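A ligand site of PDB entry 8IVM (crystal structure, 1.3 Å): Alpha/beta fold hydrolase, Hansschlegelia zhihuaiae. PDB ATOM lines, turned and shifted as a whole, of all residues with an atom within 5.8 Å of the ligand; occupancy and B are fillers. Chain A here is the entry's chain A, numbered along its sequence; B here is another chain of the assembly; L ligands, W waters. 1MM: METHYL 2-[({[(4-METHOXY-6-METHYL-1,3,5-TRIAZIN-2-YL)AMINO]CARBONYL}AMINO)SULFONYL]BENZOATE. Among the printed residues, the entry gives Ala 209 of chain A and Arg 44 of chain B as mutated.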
ATOM      1  N   GLY A  77      28.698   1.949   6.282  1.00  0.00           N
ATOM      2  CA  GLY A  77      27.497   2.017   7.090  1.00  0.00           C
ATOM      3  C   GLY A  77      26.834   3.383   7.077  1.00  0.00           C
ATOM      4  O   GLY A  77      27.137   4.254   6.252  1.00  0.00           O
ATOM      5  N   GLY A  78      25.884   3.553   7.989  1.00  0.00           N
ATOM      6  CA  GLY A  78      25.026   4.726   7.954  1.00  0.00           C
ATOM      7  C   GLY A  78      25.814   5.995   8.233  1.00  0.00           C
ATOM      8  O   GLY A  78      26.601   6.056   9.175  1.00  0.00           O
ATOM      9  N   GLY A  79      25.573   7.016   7.418  1.00  0.00           N
ATOM     10  CA  GLY A  79      26.209   8.303   7.604  1.00  0.00           C
ATOM     11  C   GLY A  79      27.680   8.338   7.276  1.00  0.00           C
ATOM     12  O   GLY A  79      28.372   9.282   7.664  1.00  0.00           O
ATOM     13  N   LEU A  80      28.181   7.335   6.541  1.00  0.00           N
ATOM     14  CA  LEU A  80      29.612   7.182   6.285  1.00  0.00           C
ATOM     15  C   LEU A  80      29.893   7.270   4.794  1.00  0.00           C
ATOM     16  O   LEU A  80      29.014   7.555   3.982  1.00  0.00           O
ATOM     17  CB  LEU A  80      30.122   5.871   6.898  1.00  0.00           C
ATOM     18  CG  LEU A  80      29.872   5.766   8.400  1.00  0.00           C
ATOM     19  CD1 LEU A  80      29.991   4.320   8.841  1.00  0.00           C
ATOM     20  CD2 LEU A  80      30.866   6.660   9.134  1.00  0.00           C
ATOM     21  N   GLY A 140      17.780  14.675   9.697  1.00  0.00           N
ATOM     22  CA  GLY A 140      18.227  14.153  10.976  1.00  0.00           C
ATOM     23  C   GLY A 140      19.704  13.838  10.901  1.00  0.00           C
ATOM     24  O   GLY A 140      20.272  13.648   9.828  1.00  0.00           O
ATOM     25  N   ASN A 141      20.350  13.791  12.070  1.00  0.00           N
ATOM     26  CA  ASN A 141      21.784  13.523  12.097  1.00  0.00           C
ATOM     27  C   ASN A 141      22.178  13.129  13.505  1.00  0.00           C
ATOM     28  O   ASN A 141      21.725  13.741  14.476  1.00  0.00           O
ATOM     29  CB  ASN A 141      22.563  14.769  11.665  1.00  0.00           C
ATOM     30  CG  ASN A 141      24.007  14.478  11.294  1.00  0.00           C
ATOM     31  OD1 ASN A 141      24.433  13.315  11.219  1.00  0.00           O
ATOM     32  ND2 ASN A 141      24.778  15.529  11.061  1.00  0.00           N
ATOM     33  N   SER A 142      23.043  12.132  13.607  1.00  0.00           N
ATOM     34  CA  SER A 142      23.570  11.753  14.903  1.00  0.00           C
ATOM     35  C   SER A 142      24.505  12.846  15.421  1.00  0.00           C
ATOM     36  O   SER A 142      25.069  13.628  14.670  1.00  0.00           O
ATOM     37  CB  SER A 142      24.359  10.444  14.809  1.00  0.00           C
ATOM     38  OG  SER A 142      24.853  10.046  16.085  1.00  0.00           O
ATOM     39  N   SER A 143      24.656  12.886  16.740  1.00  0.00           N
ATOM     40  CA  SER A 143      25.675  13.708  17.368  1.00  0.00           C
ATOM     41  C   SER A 143      26.907  12.876  17.661  1.00  0.00           C
ATOM     42  O   SER A 143      26.912  11.645  17.544  1.00  0.00           O
ATOM     43  CB  SER A 143      25.124  14.267  18.680  1.00  0.00           C
ATOM     44  OG  SER A 143      24.867  13.202  19.578  1.00  0.00           O
ATOM     45  N   GLY A 146      25.892  10.568  20.504  1.00  0.00           N
ATOM     46  CA  GLY A 146      25.128   9.429  20.050  1.00  0.00           C
ATOM     47  C   GLY A 146      25.983   8.403  19.346  1.00  0.00           C
ATOM     48  O   GLY A 146      25.838   7.197  19.560  1.00  0.00           O
ATOM     49  N   ALA A 147      26.890   8.856  18.491  1.00  0.00           N
ATOM     50  CA  ALA A 147      27.748   7.919  17.768  1.00  0.00           C
ATOM     51  C   ALA A 147      28.719   7.219  18.703  1.00  0.00           C
ATOM     52  O   ALA A 147      29.025   6.046  18.500  1.00  0.00           O
ATOM     53  CB  ALA A 147      28.510   8.652  16.656  1.00  0.00           C
ATOM     54  N   ARG A 150      26.595   4.480  20.176  1.00  0.00           N
ATOM     55  CA  ARG A 150      26.211   3.600  19.073  1.00  0.00           C
ATOM     56  C   ARG A 150      27.341   2.684  18.655  1.00  0.00           C
ATOM     57  O   ARG A 150      27.121   1.500  18.366  1.00  0.00           O
ATOM     58  CB  ARG A 150      25.798   4.467  17.889  1.00  0.00           C
ATOM     59  CG  ARG A 150      25.394   3.692  16.647  1.00  0.00           C
ATOM     60  CD  ARG A 150      25.360   4.617  15.446  1.00  0.00           C
ATOM     61  NE  ARG A 150      26.705   4.986  15.016  1.00  0.00           N
ATOM     62  CZ  ARG A 150      26.976   5.918  14.098  1.00  0.00           C
ATOM     63  NH1 ARG A 150      25.998   6.595  13.516  1.00  0.00           N
ATOM     64  NH2 ARG A 150      28.232   6.158  13.769  1.00  0.00           N
ATOM     65  N   ASP A 151      28.555   3.216  18.586  1.00  0.00           N
ATOM     66  CA  ASP A 151      29.687   2.438  18.088  1.00  0.00           C
ATOM     67  C   ASP A 151      30.399   1.680  19.189  1.00  0.00           C
ATOM     68  O   ASP A 151      31.361   0.956  18.913  1.00  0.00           O
ATOM     69  CB  ASP A 151      30.628   3.360  17.301  1.00  0.00           C
ATOM     70  CG  ASP A 151      29.923   4.013  16.109  1.00  0.00           C
ATOM     71  OD1 ASP A 151      28.871   3.467  15.694  1.00  0.00           O
ATOM     72  OD2 ASP A 151      30.396   5.051  15.590  1.00  0.00           O
ATOM     73  N   HIS A 208      28.263  -3.057   6.347  1.00  0.00           N
ATOM     74  CA  HIS A 208      28.494  -2.504   7.676  1.00  0.00           C
ATOM     75  C   HIS A 208      27.257  -1.840   8.176  1.00  0.00           C
ATOM     76  O   HIS A 208      26.732  -0.992   7.532  1.00  0.00           O
ATOM     77  CB  HIS A 208      29.586  -1.413   7.573  1.00  0.00           C
ATOM     78  CG  HIS A 208      29.863  -0.709   8.848  1.00  0.00           C
ATOM     79  ND1 HIS A 208      30.071   0.654   8.913  1.00  0.00           N
ATOM     80  CD2 HIS A 208      30.013  -1.170  10.108  1.00  0.00           C
ATOM     81  CE1 HIS A 208      30.315   0.993  10.166  1.00  0.00           C
ATOM     82  NE2 HIS A 208      30.291  -0.092  10.905  1.00  0.00           N
ATOM     83  N   ALA A 209      26.828  -2.229   9.360  1.00  0.00           N
ATOM     84  CA  ALA A 209      25.723  -1.511  10.006  1.00  0.00           C
ATOM     85  C   ALA A 209      24.509  -1.251   9.102  1.00  0.00           C
ATOM     86  O   ALA A 209      23.897  -2.186   8.707  1.00  0.00           O
ATOM     87  CB  ALA A 209      26.254  -0.261  10.718  1.00  0.00           C
ATOM     88  N   ALA A 210      24.238   0.008   8.806  1.00  0.00           N
ATOM     89  CA  ALA A 210      23.065   0.319   7.984  1.00  0.00           C
ATOM     90  C   ALA A 210      23.083  -0.380   6.636  1.00  0.00           C
ATOM     91  O   ALA A 210      22.013  -0.647   6.066  1.00  0.00           O
ATOM     92  CB  ALA A 210      22.928   1.819   7.764  1.00  0.00           C
ATOM     93  N   SER A 211      24.260  -0.673   6.073  1.00  0.00           N
ATOM     94  CA  SER A 211      24.240  -1.318   4.762  1.00  0.00           C
ATOM     95  C   SER A 211      24.037  -2.825   4.838  1.00  0.00           C
ATOM     96  O   SER A 211      23.884  -3.456   3.788  1.00  0.00           O
ATOM     97  CB  SER A 211      25.482  -0.950   3.932  1.00  0.00           C
ATOM     98  OG  SER A 211      26.637  -1.504   4.486  1.00  0.00           O
ATOM     99  N   GLU A 232      28.499  -5.923  11.964  1.00  0.00           N
ATOM    100  CA  GLU A 232      27.566  -5.250  12.876  1.00  0.00           C
ATOM    101  C   GLU A 232      26.324  -4.732  12.161  1.00  0.00           C
ATOM    102  O   GLU A 232      25.986  -3.548  12.258  1.00  0.00           O
ATOM    103  CB  GLU A 232      28.270  -4.124  13.627  1.00  0.00           C
ATOM    104  CG  GLU A 232      29.494  -4.563  14.384  1.00  0.00           C
ATOM    105  CD  GLU A 232      29.255  -4.570  15.874  1.00  0.00           C
ATOM    106  OE1 GLU A 232      28.217  -4.038  16.330  1.00  0.00           O
ATOM    107  OE2 GLU A 232      30.102  -5.114  16.603  1.00  0.00           O
ATOM    108  N   ALA A 234      22.702  -3.472  11.191  1.00  0.00           N
ATOM    109  CA  ALA A 234      21.808  -2.715  12.049  1.00  0.00           C
ATOM    110  C   ALA A 234      20.348  -3.156  11.976  1.00  0.00           C
ATOM    111  O   ALA A 234      19.618  -2.966  12.958  1.00  0.00           O
ATOM    112  CB  ALA A 234      21.888  -1.214  11.729  1.00  0.00           C
ATOM    113  N   PHE A 257      15.217  -1.878  15.529  1.00  0.00           N
ATOM    114  CA  PHE A 257      14.645  -1.431  14.261  1.00  0.00           C
ATOM    115  C   PHE A 257      13.677  -2.488  13.757  1.00  0.00           C
ATOM    116  O   PHE A 257      13.989  -3.686  13.817  1.00  0.00           O
ATOM    117  CB  PHE A 257      15.751  -1.233  13.220  1.00  0.00           C
ATOM    118  CG  PHE A 257      16.621  -0.023  13.457  1.00  0.00           C
ATOM    119  CD1 PHE A 257      16.290   0.917  14.416  1.00  0.00           C
ATOM    120  CD2 PHE A 257      17.788   0.148  12.723  1.00  0.00           C
ATOM    121  CE1 PHE A 257      17.105   2.025  14.627  1.00  0.00           C
ATOM    122  CE2 PHE A 257      18.594   1.248  12.925  1.00  0.00           C
ATOM    123  CZ  PHE A 257      18.259   2.188  13.875  1.00  0.00           C
ATOM    124  N   PHE A 293      22.094   2.003  24.132  1.00  0.00           N
ATOM    125  CA  PHE A 293      22.649   1.435  22.913  1.00  0.00           C
ATOM    126  C   PHE A 293      23.329   0.083  23.112  1.00  0.00           C
ATOM    127  O   PHE A 293      23.328  -0.718  22.235  1.00  0.00           O
ATOM    128  CB  PHE A 293      23.538   2.467  22.158  1.00  0.00           C
ATOM    129  CG  PHE A 293      23.081   2.711  20.757  1.00  0.00           C
ATOM    130  CD1 PHE A 293      22.929   1.666  19.863  1.00  0.00           C
ATOM    131  CD2 PHE A 293      22.791   3.979  20.330  1.00  0.00           C
ATOM    132  CE1 PHE A 293      22.502   1.889  18.578  1.00  0.00           C
ATOM    133  CE2 PHE A 293      22.345   4.214  19.041  1.00  0.00           C
ATOM    134  CZ  PHE A 293      22.203   3.168  18.175  1.00  0.00           C
ATOM    135  N   TRP A 296      20.381  -2.119  23.028  1.00  0.00           N
ATOM    136  CA  TRP A 296      19.910  -2.185  21.654  1.00  0.00           C
ATOM    137  C   TRP A 296      20.719  -3.197  20.871  1.00  0.00           C
ATOM    138  O   TRP A 296      20.172  -3.964  20.139  1.00  0.00           O
ATOM    139  CB  TRP A 296      19.967  -0.788  21.031  1.00  0.00           C
ATOM    140  CG  TRP A 296      19.397  -0.648  19.657  1.00  0.00           C
ATOM    141  CD1 TRP A 296      18.174  -0.196  19.347  1.00  0.00           C
ATOM    142  CD2 TRP A 296      20.059  -0.918  18.409  1.00  0.00           C
ATOM    143  NE1 TRP A 296      17.997  -0.165  17.997  1.00  0.00           N
ATOM    144  CE2 TRP A 296      19.145  -0.603  17.388  1.00  0.00           C
ATOM    145  CE3 TRP A 296      21.325  -1.381  18.054  1.00  0.00           C
ATOM    146  CZ2 TRP A 296      19.456  -0.756  16.047  1.00  0.00           C
ATOM    147  CZ3 TRP A 296      21.628  -1.529  16.716  1.00  0.00           C
ATOM    148  CH2 TRP A 296      20.704  -1.213  15.731  1.00  0.00           C
ATOM    149  N   TRP A 297      22.030  -3.161  21.027  1.00  0.00           N
ATOM    150  CA  TRP A 297      22.895  -4.130  20.342  1.00  0.00           C
ATOM    151  C   TRP A 297      22.670  -5.571  20.811  1.00  0.00           C
ATOM    152  O   TRP A 297      22.747  -6.462  20.031  1.00  0.00           O
ATOM    153  CB  TRP A 297      24.381  -3.759  20.446  1.00  0.00           C
ATOM    154  CG  TRP A 297      24.819  -2.717  19.461  1.00  0.00           C
ATOM    155  CD1 TRP A 297      25.243  -1.458  19.743  1.00  0.00           C
ATOM    156  CD2 TRP A 297      24.864  -2.839  18.036  1.00  0.00           C
ATOM    157  NE1 TRP A 297      25.553  -0.798  18.590  1.00  0.00           N
ATOM    158  CE2 TRP A 297      25.325  -1.624  17.528  1.00  0.00           C
ATOM    159  CE3 TRP A 297      24.558  -3.869  17.145  1.00  0.00           C
ATOM    160  CZ2 TRP A 297      25.500  -1.396  16.174  1.00  0.00           C
ATOM    161  CZ3 TRP A 297      24.721  -3.645  15.796  1.00  0.00           C
ATOM    162  CH2 TRP A 297      25.175  -2.419  15.322  1.00  0.00           C
ATOM    163  N   PHE A 334      33.075  -0.698  14.432  1.00  0.00           N
ATOM    164  CA  PHE A 334      33.849  -0.476  13.182  1.00  0.00           C
ATOM    165  C   PHE A 334      35.143  -1.326  13.335  1.00  0.00           C
ATOM    166  O   PHE A 334      36.215  -0.803  13.381  1.00  0.00           O
ATOM    167  CB  PHE A 334      34.305   0.986  13.013  1.00  0.00           C
ATOM    168  CG  PHE A 334      33.210   1.985  12.675  1.00  0.00           C
ATOM    169  CD1 PHE A 334      31.995   2.022  13.338  1.00  0.00           C
ATOM    170  CD2 PHE A 334      33.473   2.968  11.741  1.00  0.00           C
ATOM    171  CE1 PHE A 334      31.051   2.982  13.030  1.00  0.00           C
ATOM    172  CE2 PHE A 334      32.540   3.935  11.450  1.00  0.00           C
ATOM    173  CZ  PHE A 334      31.332   3.953  12.099  1.00  0.00           C
ATOM    174  N   VAL B  42      18.462   6.764  22.207  1.00  0.00           N
ATOM    175  CA  VAL B  42      19.498   7.590  21.606  1.00  0.00           C
ATOM    176  C   VAL B  42      19.076   8.182  20.267  1.00  0.00           C
ATOM    177  O   VAL B  42      19.539   9.267  19.902  1.00  0.00           O
ATOM    178  CB  VAL B  42      20.817   6.799  21.519  1.00  0.00           C
ATOM    179  CG1 VAL B  42      21.885   7.585  20.744  1.00  0.00           C
ATOM    180  CG2 VAL B  42      21.330   6.459  22.907  1.00  0.00           C
ATOM    181  N   ILE B  43      18.185   7.514  19.556  1.00  0.00           N
ATOM    182  CA  ILE B  43      17.831   7.890  18.186  1.00  0.00           C
ATOM    183  C   ILE B  43      16.556   8.721  18.248  1.00  0.00           C
ATOM    184  O   ILE B  43      15.441   8.212  18.134  1.00  0.00           O
ATOM    185  CB  ILE B  43      17.732   6.660  17.298  1.00  0.00           C
ATOM    186  CG1 ILE B  43      19.092   5.954  17.295  1.00  0.00           C
ATOM    187  CG2 ILE B  43      17.294   7.031  15.884  1.00  0.00           C
ATOM    188  CD1 ILE B  43      19.095   4.584  16.695  1.00  0.00           C
ATOM    189  N   ARG B  44      16.739  10.034  18.407  1.00  0.00           N
ATOM    190  CA  ARG B  44      15.653  10.970  18.638  1.00  0.00           C
ATOM    191  C   ARG B  44      15.808  12.164  17.707  1.00  0.00           C
ATOM    192  O   ARG B  44      16.930  12.555  17.358  1.00  0.00           O
ATOM    193  CB  ARG B  44      15.691  11.497  20.078  1.00  0.00           C
ATOM    194  CG  ARG B  44      15.424  10.444  21.128  1.00  0.00           C
ATOM    195  CD  ARG B  44      15.488  10.999  22.549  1.00  0.00           C
ATOM    196  NE  ARG B  44      15.311  12.448  22.618  1.00  0.00           N
ATOM    197  CZ  ARG B  44      16.000  13.248  23.428  1.00  0.00           C
ATOM    198  NH1 ARG B  44      15.760  14.547  23.441  1.00  0.00           N
ATOM    199  NH2 ARG B  44      16.928  12.741  24.236  1.00  0.00           N
ATOM    200  N   TYR B  45      14.682  12.738  17.292  1.00  0.00           N
ATOM    201  CA  TYR B  45      14.673  14.003  16.572  1.00  0.00           C
ATOM    202  C   TYR B  45      14.964  15.113  17.578  1.00  0.00           C
ATOM    203  O   TYR B  45      14.072  15.799  18.071  1.00  0.00           O
ATOM    204  CB  TYR B  45      13.336  14.226  15.881  1.00  0.00           C
ATOM    205  CG  TYR B  45      13.261  15.520  15.100  1.00  0.00           C
ATOM    206  CD1 TYR B  45      14.127  15.782  14.051  1.00  0.00           C
ATOM    207  CD2 TYR B  45      12.324  16.475  15.417  1.00  0.00           C
ATOM    208  CE1 TYR B  45      14.039  16.965  13.336  1.00  0.00           C
ATOM    209  CE2 TYR B  45      12.238  17.659  14.710  1.00  0.00           C
ATOM    210  CZ  TYR B  45      13.092  17.895  13.676  1.00  0.00           C
ATOM    211  OH  TYR B  45      12.964  19.088  13.007  1.00  0.00           O
ATOM    212  N   SER B  46      16.245  15.248  17.907  1.00  0.00           N
ATOM    213  CA  SER B  46      16.633  16.185  18.947  1.00  0.00           C
ATOM    214  C   SER B  46      18.102  16.533  18.811  1.00  0.00           C
ATOM    215  O   SER B  46      18.935  15.684  18.461  1.00  0.00           O
ATOM    216  CB  SER B  46      16.388  15.601  20.335  1.00  0.00           C
ATOM    217  OG  SER B  46      16.661  16.555  21.342  1.00  0.00           O
ATOM    218  N   ASN B 123      19.297  18.042  13.261  1.00  0.00           N
ATOM    219  CA  ASN B 123      17.930  17.570  13.387  1.00  0.00           C
ATOM    220  C   ASN B 123      17.029  18.796  13.306  1.00  0.00           C
ATOM    221  O   ASN B 123      16.985  19.598  14.232  1.00  0.00           O
ATOM    222  CB  ASN B 123      17.757  16.805  14.690  1.00  0.00           C
ATOM    223  CG  ASN B 123      18.689  15.633  14.783  1.00  0.00           C
ATOM    224  OD1 ASN B 123      18.463  14.614  14.150  1.00  0.00           O
ATOM    225  ND2 ASN B 123      19.783  15.795  15.510  1.00  0.00           N
HETATM  226  C4  1MM L   1      21.951   2.014  14.388  1.00  0.00           C
HETATM  227  C5  1MM L   1      23.142   1.303  14.488  1.00  0.00           C
HETATM  228  C6  1MM L   1      24.173   1.623  13.594  1.00  0.00           C
HETATM  229  C1  1MM L   1      23.974   2.610  12.614  1.00  0.00           C
HETATM  230  C2  1MM L   1      22.790   3.339  12.502  1.00  0.00           C
HETATM  231  C3  1MM L   1      21.785   3.006  13.417  1.00  0.00           C
HETATM  232  S7  1MM L   1      22.558   4.522  11.380  1.00  0.00           S
HETATM  233  N8  1MM L   1      21.546   5.610  11.962  1.00  0.00           N
HETATM  234  C9  1MM L   1      21.890   6.421  12.950  1.00  0.00           C
HETATM  235  N10 1MM L   1      21.036   7.425  13.164  1.00  0.00           N
HETATM  236  C2' 1MM L   1      21.021   8.247  14.228  1.00  0.00           C
HETATM  237  N1' 1MM L   1      20.196   9.317  14.200  1.00  0.00           N
HETATM  238  C6' 1MM L   1      20.127  10.159  15.253  1.00  0.00           C
HETATM  239  N5' 1MM L   1      20.889   9.926  16.331  1.00  0.00           N
HETATM  240  C4' 1MM L   1      21.709   8.848  16.361  1.00  0.00           C
HETATM  241  N3' 1MM L   1      21.773   7.997  15.310  1.00  0.00           N
HETATM  242  O7A 1MM L   1      23.793   5.179  11.042  1.00  0.00           O
HETATM  243  O7B 1MM L   1      21.971   3.945  10.201  1.00  0.00           O
HETATM  244  O9  1MM L   1      22.937   6.259  13.577  1.00  0.00           O
HETATM  245  C11 1MM L   1      25.111   2.868  11.681  1.00  0.00           C
HETATM  246  O12 1MM L   1      26.330   3.351  12.246  1.00  0.00           O
HETATM  247  C13 1MM L   1      27.435   3.618  11.378  1.00  0.00           C
HETATM  248  O11 1MM L   1      25.043   2.586  10.483  1.00  0.00           O
HETATM  249  O4' 1MM L   1      22.480   8.587  17.446  1.00  0.00           O
HETATM  250  C5' 1MM L   1      23.329   7.442  17.410  1.00  0.00           C
HETATM  251  C7' 1MM L   1      19.216  11.360  15.195  1.00  0.00           C
HETATM  252  O   HOH W   1      23.971   7.950  10.569  1.00  0.00           O
HETATM  253  O   HOH W   2      18.787   5.105  11.686  1.00  0.00           O
HETATM  254  O   HOH W   3      22.449  11.598  18.355  1.00  0.00           O
HETATM  255  O   HOH W   4      20.257   1.732  10.087  1.00  0.00           O
HETATM  256  O   HOH W   5      21.371   6.451   8.118  1.00  0.00           O
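Water W3 bridges the backbone NH (N) of Ser 143 (3.0 Å) and a nitrogen (N5') of the ligand (3.1 Å).
N of Gly 146 is in hydrogen-bond range of OG of Ser 143, at 3.0 Å.
ND2 of Asn 123 of chain B lies within hydrogen-bond range of O of Ser 46 of chain B (3.1 Å).
OG of Ser 46 of chain B lies within hydrogen-bond range of NH1 of Arg 44 of chain B (3.0 Å).
NE of Arg 150 is in salt-bridge range of OD1 of Asp 151, 2.7 Å away.
The backbone NH (N) of Ala 209 lies close to the backbone carbonyl oxygen (O) of Glu 232, at 3.3 Å.
N of Asn 141 lies within hydrogen-bond range of OD1 of Asn 123 of chain B.
O of Arg 150 lies within hydrogen-bond range of NE1 of Trp 297 (2.8 Å).
N of Ala 147 is in hydrogen-bond range of OG of Ser 142.
The backbone NH of Gly 78 is in hydrogen-bond range of an oxygen (O11) of the ligand, 2.8 Å away.
O11 of the ligand sits at hydrogen-bond distance from N of Ala 210.
OG of Ser 142 is in hydrogen-bond range of O4' of the ligand.
NH1 of Arg 150 is in hydrogen-bond range of O9 of the ligand, 3.1 Å away.
Gly 77 touches the ligand.
CD1 of Leu 80 touches C13 of the ligand, 3.7 Å away.
O of Asn 141 touches C7' of the ligand (3.5 Å).
Gly 146 touches the ligand (O to C5', 3.3 Å).
Ala 147 touches the ligand.
Ala 209 touches the ligand.
CB of Ala 234 touches C5 of the ligand (3.9 Å).
Phe 257 touches the ligand.
Phe 293 touches the ligand.
CH2 of Trp 296 touches C4 of the ligand, at 3.7 Å.
Trp 297 touches the ligand.
Phe 334 touches the ligand.
CG1 of Val 42 of chain B touches O4' of the ligand, 3.5 Å away.
Ile 43 of chain B touches the ligand (CG1 to N3', 3.9 Å).
Arg 44 of chain B touches the ligand (O to C7', 3.4 Å).
OD1 of Asn 123 of chain B touches C7' of the ligand, 3.5 Å away.
20 residues have an atom within 4 Å of the ligand: Gly 77, Gly 78, Leu 80, Asn 141, Ser 142, Gly 146, Ala 147, Arg 150, Ala 209, Ala 210, Ala 234, Phe 257, Phe 293, Trp 296, Trp 297, Phe 334, Val 42 of chain B, Ile 43 of chain B, Arg 44 of chain B and Asn 123 of chain B.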
